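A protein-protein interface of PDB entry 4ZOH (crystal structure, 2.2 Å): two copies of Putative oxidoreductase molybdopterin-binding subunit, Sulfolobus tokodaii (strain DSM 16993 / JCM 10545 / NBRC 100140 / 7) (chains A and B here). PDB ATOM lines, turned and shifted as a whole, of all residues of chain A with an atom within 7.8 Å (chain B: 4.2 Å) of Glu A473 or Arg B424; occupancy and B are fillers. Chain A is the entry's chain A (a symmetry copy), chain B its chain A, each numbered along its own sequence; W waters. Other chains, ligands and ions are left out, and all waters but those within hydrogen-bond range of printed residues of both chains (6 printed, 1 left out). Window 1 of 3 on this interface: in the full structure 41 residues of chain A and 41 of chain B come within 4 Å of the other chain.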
ATOM      1  N   LYS A 178      25.790  17.601  -0.051  1.00  0.00           N
ATOM      2  CA  LYS A 178      25.266  17.530   1.297  1.00  0.00           C
ATOM      3  C   LYS A 178      26.343  17.872   2.359  1.00  0.00           C
ATOM      4  O   LYS A 178      27.483  17.354   2.324  1.00  0.00           O
ATOM      5  CB  LYS A 178      24.731  16.141   1.428  1.00  0.00           C
ATOM      6  CG  LYS A 178      24.270  15.767   2.777  1.00  0.00           C
ATOM      7  CD  LYS A 178      23.894  14.307   2.586  1.00  0.00           C
ATOM      8  CE  LYS A 178      23.538  13.645   3.879  1.00  0.00           C
ATOM      9  NZ  LYS A 178      23.039  12.290   3.480  1.00  0.00           N
ATOM     10  N   LEU A 179      25.958  18.713   3.303  1.00  0.00           N
ATOM     11  CA  LEU A 179      26.770  18.974   4.488  1.00  0.00           C
ATOM     12  C   LEU A 179      26.439  17.967   5.578  1.00  0.00           C
ATOM     13  O   LEU A 179      25.302  17.870   5.996  1.00  0.00           O
ATOM     14  CB  LEU A 179      26.495  20.359   5.074  1.00  0.00           C
ATOM     15  CG  LEU A 179      27.324  20.846   6.286  1.00  0.00           C
ATOM     16  CD1 LEU A 179      28.804  20.732   6.094  1.00  0.00           C
ATOM     17  CD2 LEU A 179      26.892  22.260   6.657  1.00  0.00           C
ATOM     18  N   THR A 180      27.441  17.230   6.043  1.00  0.00           N
ATOM     19  CA  THR A 180      27.244  16.459   7.324  1.00  0.00           C
ATOM     20  C   THR A 180      27.988  17.201   8.427  1.00  0.00           C
ATOM     21  O   THR A 180      29.134  17.559   8.207  1.00  0.00           O
ATOM     22  CB  THR A 180      27.710  15.006   7.182  1.00  0.00           C
ATOM     23  OG1 THR A 180      26.942  14.398   6.138  1.00  0.00           O
ATOM     24  CG2 THR A 180      27.490  14.241   8.452  1.00  0.00           C
ATOM     25  N   ALA A 188      20.431  17.774  17.736  1.00  0.00           N
ATOM     26  CA  ALA A 188      20.838  17.699  16.308  1.00  0.00           C
ATOM     27  C   ALA A 188      19.797  18.444  15.378  1.00  0.00           C
ATOM     28  O   ALA A 188      20.179  19.141  14.484  1.00  0.00           O
ATOM     29  CB  ALA A 188      21.033  16.265  15.868  1.00  0.00           C
ATOM     30  N   HIS A 189      18.508  18.324  15.667  1.00  0.00           N
ATOM     31  CA  HIS A 189      17.464  18.776  14.773  1.00  0.00           C
ATOM     32  C   HIS A 189      17.363  20.288  14.793  1.00  0.00           C
ATOM     33  O   HIS A 189      17.196  20.887  13.720  1.00  0.00           O
ATOM     34  CB  HIS A 189      16.145  18.091  15.141  1.00  0.00           C
ATOM     35  CG  HIS A 189      16.301  16.618  15.384  1.00  0.00           C
ATOM     36  ND1 HIS A 189      16.345  15.697  14.352  1.00  0.00           N
ATOM     37  CD2 HIS A 189      16.422  15.902  16.536  1.00  0.00           C
ATOM     38  CE1 HIS A 189      16.484  14.474  14.862  1.00  0.00           C
ATOM     39  NE2 HIS A 189      16.528  14.569  16.181  1.00  0.00           N
ATOM     40  N   ARG A 192      20.403  21.619  13.054  1.00  0.00           N
ATOM     41  CA  ARG A 192      20.191  21.555  11.643  1.00  0.00           C
ATOM     42  C   ARG A 192      19.339  22.765  11.111  1.00  0.00           C
ATOM     43  O   ARG A 192      19.708  23.385  10.104  1.00  0.00           O
ATOM     44  CB  ARG A 192      19.495  20.274  11.271  1.00  0.00           C
ATOM     45  CG  ARG A 192      19.431  20.125   9.768  1.00  0.00           C
ATOM     46  CD  ARG A 192      18.643  18.905   9.364  1.00  0.00           C
ATOM     47  NE  ARG A 192      18.129  19.179   8.027  1.00  0.00           N
ATOM     48  CZ  ARG A 192      16.984  19.841   7.781  1.00  0.00           C
ATOM     49  NH1 ARG A 192      16.196  20.255   8.796  1.00  0.00           N
ATOM     50  NH2 ARG A 192      16.628  20.096   6.500  1.00  0.00           N
ATOM     51  N   ASN A 203      19.965  20.564   2.488  1.00  0.00           N
ATOM     52  CA  ASN A 203      20.622  19.257   2.448  1.00  0.00           C
ATOM     53  C   ASN A 203      21.728  19.112   3.466  1.00  0.00           C
ATOM     54  O   ASN A 203      22.918  19.136   3.116  1.00  0.00           O
ATOM     55  CB  ASN A 203      21.073  18.901   1.037  1.00  0.00           C
ATOM     56  CG  ASN A 203      20.099  17.988   0.390  1.00  0.00           C
ATOM     57  OD1 ASN A 203      19.316  18.419  -0.435  1.00  0.00           O
ATOM     58  ND2 ASN A 203      20.089  16.707   0.822  1.00  0.00           N
ATOM     59  N   ILE A 204      21.294  19.135   4.728  1.00  0.00           N
ATOM     60  CA  ILE A 204      22.198  19.165   5.861  1.00  0.00           C
ATOM     61  C   ILE A 204      21.755  18.017   6.785  1.00  0.00           C
ATOM     62  O   ILE A 204      20.577  17.910   7.107  1.00  0.00           O
ATOM     63  CB  ILE A 204      22.142  20.488   6.595  1.00  0.00           C
ATOM     64  CG1 ILE A 204      22.421  21.677   5.595  1.00  0.00           C
ATOM     65  CG2 ILE A 204      23.099  20.480   7.800  1.00  0.00           C
ATOM     66  CD1 ILE A 204      22.645  23.003   6.320  1.00  0.00           C
ATOM     67  N   ARG A 205      22.688  17.107   7.072  1.00  0.00           N
ATOM     68  CA  ARG A 205      22.499  16.107   8.137  1.00  0.00           C
ATOM     69  C   ARG A 205      23.310  16.572   9.371  1.00  0.00           C
ATOM     70  O   ARG A 205      24.500  16.901   9.237  1.00  0.00           O
ATOM     71  CB  ARG A 205      23.082  14.778   7.662  1.00  0.00           C
ATOM     72  CG  ARG A 205      23.003  13.674   8.733  1.00  0.00           C
ATOM     73  CD  ARG A 205      23.706  12.429   8.230  1.00  0.00           C
ATOM     74  NE  ARG A 205      23.289  11.223   8.935  1.00  0.00           N
ATOM     75  CZ  ARG A 205      23.585   9.984   8.511  1.00  0.00           C
ATOM     76  NH1 ARG A 205      24.296   9.817   7.409  1.00  0.00           N
ATOM     77  NH2 ARG A 205      23.157   8.912   9.170  1.00  0.00           N
ATOM     78  N   VAL A 206      22.695  16.563  10.549  1.00  0.00           N
ATOM     79  CA  VAL A 206      23.369  16.875  11.784  1.00  0.00           C
ATOM     80  C   VAL A 206      23.417  15.588  12.674  1.00  0.00           C
ATOM     81  O   VAL A 206      22.470  14.824  12.750  1.00  0.00           O
ATOM     82  CB  VAL A 206      22.785  18.105  12.531  1.00  0.00           C
ATOM     83  CG1 VAL A 206      23.532  18.318  13.825  1.00  0.00           C
ATOM     84  CG2 VAL A 206      23.078  19.402  11.692  1.00  0.00           C
ATOM     85  N   ILE A 207      24.547  15.386  13.322  1.00  0.00           N
ATOM     86  CA  ILE A 207      24.747  14.264  14.239  1.00  0.00           C
ATOM     87  C   ILE A 207      25.201  14.852  15.562  1.00  0.00           C
ATOM     88  O   ILE A 207      26.239  15.505  15.624  1.00  0.00           O
ATOM     89  CB  ILE A 207      25.769  13.249  13.684  1.00  0.00           C
ATOM     90  CG1 ILE A 207      25.174  12.586  12.427  1.00  0.00           C
ATOM     91  CG2 ILE A 207      26.134  12.193  14.760  1.00  0.00           C
ATOM     92  CD1 ILE A 207      26.116  11.689  11.659  1.00  0.00           C
ATOM     93  N   ARG A 424      10.013   7.768  17.133  1.00  0.00           N
ATOM     94  CA  ARG A 424       9.787   6.765  16.104  1.00  0.00           C
ATOM     95  C   ARG A 424      10.022   5.389  16.748  1.00  0.00           C
ATOM     96  O   ARG A 424      10.994   5.257  17.457  1.00  0.00           O
ATOM     97  CB  ARG A 424      10.761   7.021  14.906  1.00  0.00           C
ATOM     98  CG  ARG A 424      11.053   5.834  14.014  1.00  0.00           C
ATOM     99  CD  ARG A 424      11.988   6.150  12.856  1.00  0.00           C
ATOM    100  NE  ARG A 424      12.207   4.916  12.067  1.00  0.00           N
ATOM    101  CZ  ARG A 424      13.380   4.386  11.726  1.00  0.00           C
ATOM    102  NH1 ARG A 424      14.530   4.976  12.015  1.00  0.00           N
ATOM    103  NH2 ARG A 424      13.388   3.272  11.032  1.00  0.00           N
ATOM    104  N   VAL A 436      13.418   5.549  18.643  1.00  0.00           N
ATOM    105  CA  VAL A 436      14.227   6.766  18.418  1.00  0.00           C
ATOM    106  C   VAL A 436      13.494   7.942  19.041  1.00  0.00           C
ATOM    107  O   VAL A 436      12.239   8.055  18.939  1.00  0.00           O
ATOM    108  CB  VAL A 436      14.547   7.005  16.910  1.00  0.00           C
ATOM    109  CG1 VAL A 436      15.560   8.141  16.754  1.00  0.00           C
ATOM    110  CG2 VAL A 436      15.013   5.732  16.201  1.00  0.00           C
ATOM    111  N   GLY A 470      19.726  11.689  18.054  1.00  0.00           N
ATOM    112  CA  GLY A 470      20.859  12.542  17.733  1.00  0.00           C
ATOM    113  C   GLY A 470      21.406  12.420  16.309  1.00  0.00           C
ATOM    114  O   GLY A 470      22.482  12.897  16.043  1.00  0.00           O
ATOM    115  N   ASP A 471      20.632  11.833  15.408  1.00  0.00           N
ATOM    116  CA  ASP A 471      20.936  11.829  13.978  1.00  0.00           C
ATOM    117  C   ASP A 471      19.687  12.262  13.232  1.00  0.00           C
ATOM    118  O   ASP A 471      18.632  11.643  13.374  1.00  0.00           O
ATOM    119  CB  ASP A 471      21.397  10.454  13.487  1.00  0.00           C
ATOM    120  CG  ASP A 471      21.853  10.429  12.016  1.00  0.00           C
ATOM    121  OD1 ASP A 471      21.651  11.370  11.209  1.00  0.00           O
ATOM    122  OD2 ASP A 471      22.430   9.407  11.636  1.00  0.00           O
ATOM    123  N   THR A 472      19.802  13.343  12.460  1.00  0.00           N
ATOM    124  CA  THR A 472      18.631  13.900  11.728  1.00  0.00           C
ATOM    125  C   THR A 472      18.168  12.905  10.682  1.00  0.00           C
ATOM    126  O   THR A 472      17.039  13.043  10.118  1.00  0.00           O
ATOM    127  CB  THR A 472      18.952  15.279  11.088  1.00  0.00           C
ATOM    128  OG1 THR A 472      20.015  15.102  10.159  1.00  0.00           O
ATOM    129  CG2 THR A 472      19.391  16.300  12.126  1.00  0.00           C
ATOM    130  N   GLU A 473      18.961  11.856  10.423  1.00  0.00           N
ATOM    131  CA  GLU A 473      18.500  10.849   9.424  1.00  0.00           C
ATOM    132  C   GLU A 473      17.751   9.614   9.952  1.00  0.00           C
ATOM    133  O   GLU A 473      17.213   8.789   9.152  1.00  0.00           O
ATOM    134  CB  GLU A 473      19.652  10.366   8.591  1.00  0.00           C
ATOM    135  CG  GLU A 473      20.029  11.376   7.504  1.00  0.00           C
ATOM    136  CD  GLU A 473      20.776  10.777   6.319  1.00  0.00           C
ATOM    137  OE1 GLU A 473      20.665   9.530   6.077  1.00  0.00           O
ATOM    138  OE2 GLU A 473      21.457  11.587   5.626  1.00  0.00           O
ATOM    139  N   ILE A 474      17.720   9.446  11.274  1.00  0.00           N
ATOM    140  CA  ILE A 474      17.093   8.231  11.823  1.00  0.00           C
ATOM    141  C   ILE A 474      15.690   8.550  12.403  1.00  0.00           C
ATOM    142  O   ILE A 474      15.019   7.657  12.938  1.00  0.00           O
ATOM    143  CB  ILE A 474      17.978   7.536  12.876  1.00  0.00           C
ATOM    144  CG1 ILE A 474      18.119   8.442  14.089  1.00  0.00           C
ATOM    145  CG2 ILE A 474      19.334   7.129  12.299  1.00  0.00           C
ATOM    146  CD1 ILE A 474      18.957   7.861  15.209  1.00  0.00           C
ATOM    147  N   ILE A 475      15.303   9.841  12.400  1.00  0.00           N
ATOM    148  CA  ILE A 475      13.969  10.245  12.868  1.00  0.00           C
ATOM    149  C   ILE A 475      13.498  11.483  12.089  1.00  0.00           C
ATOM    150  O   ILE A 475      14.334  12.334  11.663  1.00  0.00           O
ATOM    151  CB  ILE A 475      13.921  10.446  14.411  1.00  0.00           C
ATOM    152  CG1 ILE A 475      12.451  10.510  14.954  1.00  0.00           C
ATOM    153  CG2 ILE A 475      14.815  11.578  14.886  1.00  0.00           C
ATOM    154  CD1 ILE A 475      12.321  10.548  16.468  1.00  0.00           C
ATOM    155  N   GLU A 476      12.186  11.580  11.906  1.00  0.00           N
ATOM    156  CA  GLU A 476      11.592  12.693  11.154  1.00  0.00           C
ATOM    157  C   GLU A 476      12.122  14.056  11.626  1.00  0.00           C
ATOM    158  O   GLU A 476      12.517  14.858  10.807  1.00  0.00           O
ATOM    159  CB  GLU A 476      10.060  12.661  11.183  1.00  0.00           C
ATOM    160  CG  GLU A 476       9.431  13.759  10.342  1.00  0.00           C
ATOM    161  CD  GLU A 476       7.887  13.770  10.301  1.00  0.00           C
ATOM    162  OE1 GLU A 476       7.235  13.119  11.154  1.00  0.00           O
ATOM    163  OE2 GLU A 476       7.329  14.356   9.322  1.00  0.00           O
ATOM    164  N   ASP A 477      12.169  14.319  12.933  1.00  0.00           N
ATOM    165  CA  ASP A 477      12.524  15.626  13.425  1.00  0.00           C
ATOM    166  C   ASP A 477      12.571  15.580  14.950  1.00  0.00           C
ATOM    167  O   ASP A 477      12.440  14.521  15.558  1.00  0.00           O
ATOM    168  CB  ASP A 477      11.517  16.735  12.944  1.00  0.00           C
ATOM    169  CG  ASP A 477      12.208  18.053  12.616  1.00  0.00           C
ATOM    170  OD1 ASP A 477      11.982  18.646  11.550  1.00  0.00           O
ATOM    171  OD2 ASP A 477      13.000  18.531  13.424  1.00  0.00           O
ATOM    172  N   ASP A 553       6.614   0.376  11.499  1.00  0.00           N
ATOM    173  CA  ASP A 553       7.546   1.472  11.770  1.00  0.00           C
ATOM    174  C   ASP A 553       6.604   2.643  11.966  1.00  0.00           C
ATOM    175  O   ASP A 553       5.897   2.996  11.057  1.00  0.00           O
ATOM    176  CB  ASP A 553       8.482   1.703  10.548  1.00  0.00           C
ATOM    177  CG  ASP A 553       9.673   2.620  10.878  1.00  0.00           C
ATOM    178  OD1 ASP A 553       9.517   3.677  11.560  1.00  0.00           O
ATOM    179  OD2 ASP A 553      10.804   2.247  10.522  1.00  0.00           O
ATOM    180  N   THR A 555       5.708   6.674  13.743  1.00  0.00           N
ATOM    181  CA  THR A 555       6.238   7.920  14.275  1.00  0.00           C
ATOM    182  C   THR A 555       5.100   8.690  14.897  1.00  0.00           C
ATOM    183  O   THR A 555       4.044   8.840  14.289  1.00  0.00           O
ATOM    184  CB  THR A 555       6.936   8.753  13.149  1.00  0.00           C
ATOM    185  OG1 THR A 555       8.082   8.022  12.681  1.00  0.00           O
ATOM    186  CG2 THR A 555       7.407  10.095  13.653  1.00  0.00           C
ATOM    187  N   ALA B 423      10.033   1.151   1.465  1.00  0.00           N
ATOM    188  CA  ALA B 423      10.440   2.517   1.177  1.00  0.00           C
ATOM    189  C   ALA B 423       9.928   3.342   2.335  1.00  0.00           C
ATOM    190  O   ALA B 423       8.749   3.126   2.763  1.00  0.00           O
ATOM    191  CB  ALA B 423       9.833   3.011  -0.171  1.00  0.00           C
ATOM    192  N   ARG B 424      10.758   4.284   2.803  1.00  0.00           N
ATOM    193  CA  ARG B 424      10.327   5.243   3.809  1.00  0.00           C
ATOM    194  C   ARG B 424      10.420   6.641   3.176  1.00  0.00           C
ATOM    195  O   ARG B 424      11.413   6.906   2.537  1.00  0.00           O
ATOM    196  CB  ARG B 424      11.239   5.115   5.073  1.00  0.00           C
ATOM    197  CG  ARG B 424      11.305   6.326   5.978  1.00  0.00           C
ATOM    198  CD  ARG B 424      12.190   6.133   7.200  1.00  0.00           C
ATOM    199  NE  ARG B 424      12.185   7.381   7.997  1.00  0.00           N
ATOM    200  CZ  ARG B 424      13.249   8.062   8.418  1.00  0.00           C
ATOM    201  NH1 ARG B 424      14.486   7.633   8.214  1.00  0.00           N
ATOM    202  NH2 ARG B 424      13.058   9.164   9.105  1.00  0.00           N
ATOM    203  N   ILE B 425       9.419   7.526   3.370  1.00  0.00           N
ATOM    204  CA  ILE B 425       9.587   8.911   2.957  1.00  0.00           C
ATOM    205  C   ILE B 425       9.265   9.807   4.142  1.00  0.00           C
ATOM    206  O   ILE B 425       8.286   9.598   4.826  1.00  0.00           O
ATOM    207  CB  ILE B 425       8.777   9.262   1.639  1.00  0.00           C
ATOM    208  CG1 ILE B 425       9.219  10.574   1.036  1.00  0.00           C
ATOM    209  CG2 ILE B 425       7.274   9.334   1.920  1.00  0.00           C
ATOM    210  CD1 ILE B 425       8.716  10.765  -0.425  1.00  0.00           C
ATOM    211  N   SER B 426      10.047  10.852   4.351  1.00  0.00           N
ATOM    212  CA  SER B 426       9.858  11.636   5.555  1.00  0.00           C
ATOM    213  C   SER B 426       9.986  13.122   5.301  1.00  0.00           C
ATOM    214  O   SER B 426      10.890  13.541   4.570  1.00  0.00           O
ATOM    215  CB  SER B 426      10.949  11.172   6.526  1.00  0.00           C
ATOM    216  OG  SER B 426      10.927  11.926   7.684  1.00  0.00           O
ATOM    217  N   THR B 434      13.137  13.416   2.443  1.00  0.00           N
ATOM    218  CA  THR B 434      14.085  12.312   2.243  1.00  0.00           C
ATOM    219  C   THR B 434      13.320  11.040   1.982  1.00  0.00           C
ATOM    220  O   THR B 434      12.375  10.706   2.688  1.00  0.00           O
ATOM    221  CB  THR B 434      15.016  12.135   3.489  1.00  0.00           C
ATOM    222  OG1 THR B 434      15.454  13.434   3.891  1.00  0.00           O
ATOM    223  CG2 THR B 434      16.283  11.241   3.178  1.00  0.00           C
ATOM    224  N   LEU B 435      13.734  10.375   0.918  1.00  0.00           N
ATOM    225  CA  LEU B 435      13.245   9.096   0.528  1.00  0.00           C
ATOM    226  C   LEU B 435      14.320   8.040   0.857  1.00  0.00           C
ATOM    227  O   LEU B 435      15.465   8.200   0.484  1.00  0.00           O
ATOM    228  CB  LEU B 435      12.941   9.094  -0.987  1.00  0.00           C
ATOM    229  CG  LEU B 435      12.583   7.750  -1.584  1.00  0.00           C
ATOM    230  CD1 LEU B 435      11.166   7.369  -1.159  1.00  0.00           C
ATOM    231  CD2 LEU B 435      12.668   7.866  -3.100  1.00  0.00           C
ATOM    232  N   VAL B 436      13.932   6.948   1.526  1.00  0.00           N
ATOM    233  CA  VAL B 436      14.880   5.850   1.813  1.00  0.00           C
ATOM    234  C   VAL B 436      14.356   4.588   1.146  1.00  0.00           C
ATOM    235  O   VAL B 436      13.125   4.308   1.159  1.00  0.00           O
ATOM    236  CB  VAL B 436      15.121   5.648   3.342  1.00  0.00           C
ATOM    237  CG1 VAL B 436      16.264   4.658   3.575  1.00  0.00           C
ATOM    238  CG2 VAL B 436      15.360   6.969   4.076  1.00  0.00           C
ATOM    239  N   ARG B 468      18.255   7.943  -0.112  1.00  0.00           N
ATOM    240  CA  ARG B 468      19.245   7.268   0.767  1.00  0.00           C
ATOM    241  C   ARG B 468      18.957   5.779   0.846  1.00  0.00           C
ATOM    242  O   ARG B 468      17.834   5.354   0.578  1.00  0.00           O
ATOM    243  CB  ARG B 468      19.164   7.912   2.161  1.00  0.00           C
ATOM    244  CG  ARG B 468      19.631   9.367   2.159  1.00  0.00           C
ATOM    245  CD  ARG B 468      21.156   9.416   2.175  1.00  0.00           C
ATOM    246  NE  ARG B 468      21.627   8.980   3.503  1.00  0.00           N
ATOM    247  CZ  ARG B 468      22.348   7.886   3.780  1.00  0.00           C
ATOM    248  NH1 ARG B 468      22.691   7.070   2.803  1.00  0.00           N
ATOM    249  NH2 ARG B 468      22.657   7.586   5.067  1.00  0.00           N
ATOM    250  N   ILE B 474      18.187   3.629   9.200  1.00  0.00           N
ATOM    251  CA  ILE B 474      17.443   4.751   8.602  1.00  0.00           C
ATOM    252  C   ILE B 474      16.140   4.249   7.925  1.00  0.00           C
ATOM    253  O   ILE B 474      15.393   5.046   7.341  1.00  0.00           O
ATOM    254  CB  ILE B 474      18.298   5.564   7.610  1.00  0.00           C
ATOM    255  CG1 ILE B 474      18.645   4.690   6.416  1.00  0.00           C
ATOM    256  CG2 ILE B 474      19.544   6.146   8.281  1.00  0.00           C
ATOM    257  CD1 ILE B 474      19.474   5.384   5.354  1.00  0.00           C
ATOM    258  N   ILE B 475      15.930   2.918   7.907  1.00  0.00           N
ATOM    259  CA  ILE B 475      14.698   2.341   7.348  1.00  0.00           C
ATOM    260  C   ILE B 475      14.345   1.048   8.097  1.00  0.00           C
ATOM    261  O   ILE B 475      15.256   0.314   8.585  1.00  0.00           O
ATOM    262  CB  ILE B 475      14.788   2.143   5.806  1.00  0.00           C
ATOM    263  CG1 ILE B 475      13.381   1.884   5.162  1.00  0.00           C
ATOM    264  CG2 ILE B 475      15.856   1.143   5.402  1.00  0.00           C
ATOM    265  CD1 ILE B 475      13.365   1.836   3.642  1.00  0.00           C
ATOM    266  N   ASP B 553       6.007  11.126   8.147  1.00  0.00           N
ATOM    267  CA  ASP B 553       7.094  10.166   7.948  1.00  0.00           C
ATOM    268  C   ASP B 553       6.334   8.880   7.691  1.00  0.00           C
ATOM    269  O   ASP B 553       5.618   8.432   8.549  1.00  0.00           O
ATOM    270  CB  ASP B 553       7.965  10.057   9.233  1.00  0.00           C
ATOM    271  CG  ASP B 553       9.288   9.310   8.993  1.00  0.00           C
ATOM    272  OD1 ASP B 553       9.324   8.245   8.307  1.00  0.00           O
ATOM    273  OD2 ASP B 553      10.331   9.830   9.427  1.00  0.00           O
ATOM    274  N   THR B 554       6.478   8.284   6.521  1.00  0.00           N
ATOM    275  CA  THR B 554       5.683   7.118   6.230  1.00  0.00           C
ATOM    276  C   THR B 554       6.460   6.009   5.562  1.00  0.00           C
ATOM    277  O   THR B 554       7.396   6.284   4.842  1.00  0.00           O
ATOM    278  CB  THR B 554       4.334   7.462   5.512  1.00  0.00           C
ATOM    279  OG1 THR B 554       3.476   6.307   5.607  1.00  0.00           O
ATOM    280  CG2 THR B 554       4.525   7.877   4.072  1.00  0.00           C
ATOM    281  N   THR B 555       6.116   4.774   5.874  1.00  0.00           N
ATOM    282  CA  THR B 555       6.844   3.613   5.387  1.00  0.00           C
ATOM    283  C   THR B 555       5.867   2.700   4.690  1.00  0.00           C
ATOM    284  O   THR B 555       4.801   2.407   5.223  1.00  0.00           O
ATOM    285  CB  THR B 555       7.568   2.877   6.564  1.00  0.00           C
ATOM    286  OG1 THR B 555       8.569   3.752   7.109  1.00  0.00           O
ATOM    287  CG2 THR B 555       8.249   1.612   6.101  1.00  0.00           C
HETATM  288  O   HOH W   1      10.620   9.436  12.137  1.00  0.00           O
HETATM  289  O   HOH W   2       4.562   7.423  11.149  1.00  0.00           O
HETATM  290  O   HOH W   3       4.901   3.866   8.384  1.00  0.00           O
HETATM  291  O   HOH W   4      23.640   6.463   7.529  1.00  0.00           O
HETATM  292  O   HOH W   5      15.455   1.398  11.228  1.00  0.00           O
HETATM  293  O   HOH W   6      11.228   2.689   7.838  1.00  0.00           O
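Arg A424 touches Ile B475, and with the chains exchanged Ile A475 touches Arg B424.
Positions printed for both chains: 424, 436, 474, 475, 553 and 555.
Of the 10 pairs that touch across the chains among the printed residues, 2 have their exchanged pair printed and touching as well.
Lys A178 touches Arg B468 (NZ to NE, 3.6 Å).
NH1 of Arg A205 touches NH2 of Arg B468, 3.6 Å away.
Ile B475 touches Arg A424.
Glu A473 touches Ile B474 (O to CG2, 3.6 Å).
Arg B424 touches Ile A475.
Arg B424 touches Glu A476 (NH2 to N, 3.8 Å).
Glu A476 touches Ser B426 (CG to OG, 3.6 Å).
Glu A476 touches Asp B553 (CB to OD2, 3.3 Å).
Glu A473 touches just these residues of chain B: Arg B424, Arg B468 and Ile B474.
Of chain A, only Glu A473, Ile A475 and Glu A476 come within 4 Å of Arg B424.
No residue of chain A comes within 4 Å of Ala B423.
Printed residues of chain A within 4 Å of Ile B475: Arg A424.
Of the printed residues of chain A, Asp B553 touches Glu A476 (3.3 Å).
Printed residues of chain B within 4 Å of Arg A424: Ile B475.
The nearest printed residue of chain B that does not touch Glu A473 is Thr B434 (5.5 Å).
The nearest residue of chain A that does not touch Arg B424 is Ile A474 (4.3 Å).
The nearest printed residue of chain B that does not touch Glu A476 is Ile B425 (6.6 Å).
Of the 23 printed residues of chain A, 6 touch a printed residue of chain B.
Along chain B the printed residues that touch a printed residue of chain A span positions 424 to 553.
Among the printed residues, 10 pairs touch across the chains.
Among the printed residues, Asp or Glu carboxylates within 4 Å of a Lys or Arg side-chain nitrogen of the other chain: Glu A473 with Arg B468 (2.8 Å).
Water W1 lies within hydrogen-bond range of the backbone NH (N) of Glu A476, the side-chain carboxylate (OD2) of Asp B553 and the side-chain hydroxyl (OG1) of Thr A555.
Water W6 lies within hydrogen-bond range of the side-chain carboxylate of Asp A553 and the side-chain hydroxyl of Thr B555.
Water W5 lies within hydrogen-bond range of the guanidinium group of Arg A424 (2.8 Å) and the backbone carbonyl oxygen of Ile B475 (2.9 Å).
Water W4 lies within hydrogen-bond range of NH2 of Arg B468 and NH2 of Arg A205.
Water W2 lies within hydrogen-bond range of the backbone NH of Thr A555 and the backbone carbonyl oxygen of Asp B553.
Water W3 bridges the backbone NH of Thr B555 (2.9 Å) and the backbone carbonyl oxygen of Asp A553 (3.0 Å).
The side-chain carboxylate of Glu A473 lies within salt-bridge range of the guanidinium group of Arg B468.
NH1 of Arg B424 is in hydrogen-bond range of O of Glu A473 (3.1 Å).
NH2 of Arg A424 is in salt-bridge range of OD2 of Asp A553.
The backbone carbonyl oxygen of Thr B434 lies within hydrogen-bond range of the backbone NH of Ser B426 (2.9 Å).
OD2 of Asp B553 lies within salt-bridge range of NH2 of Arg B424 (2.8 Å).
OG of Ser B426 sits at hydrogen-bond distance from OD2 of Asp B553 (2.8 Å).
NH2 of Arg A205 lies within salt-bridge range of OD2 of Asp A471, at 2.6 Å.
O of Leu A179 lies within hydrogen-bond range of N of Arg A205, 2.9 Å away.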
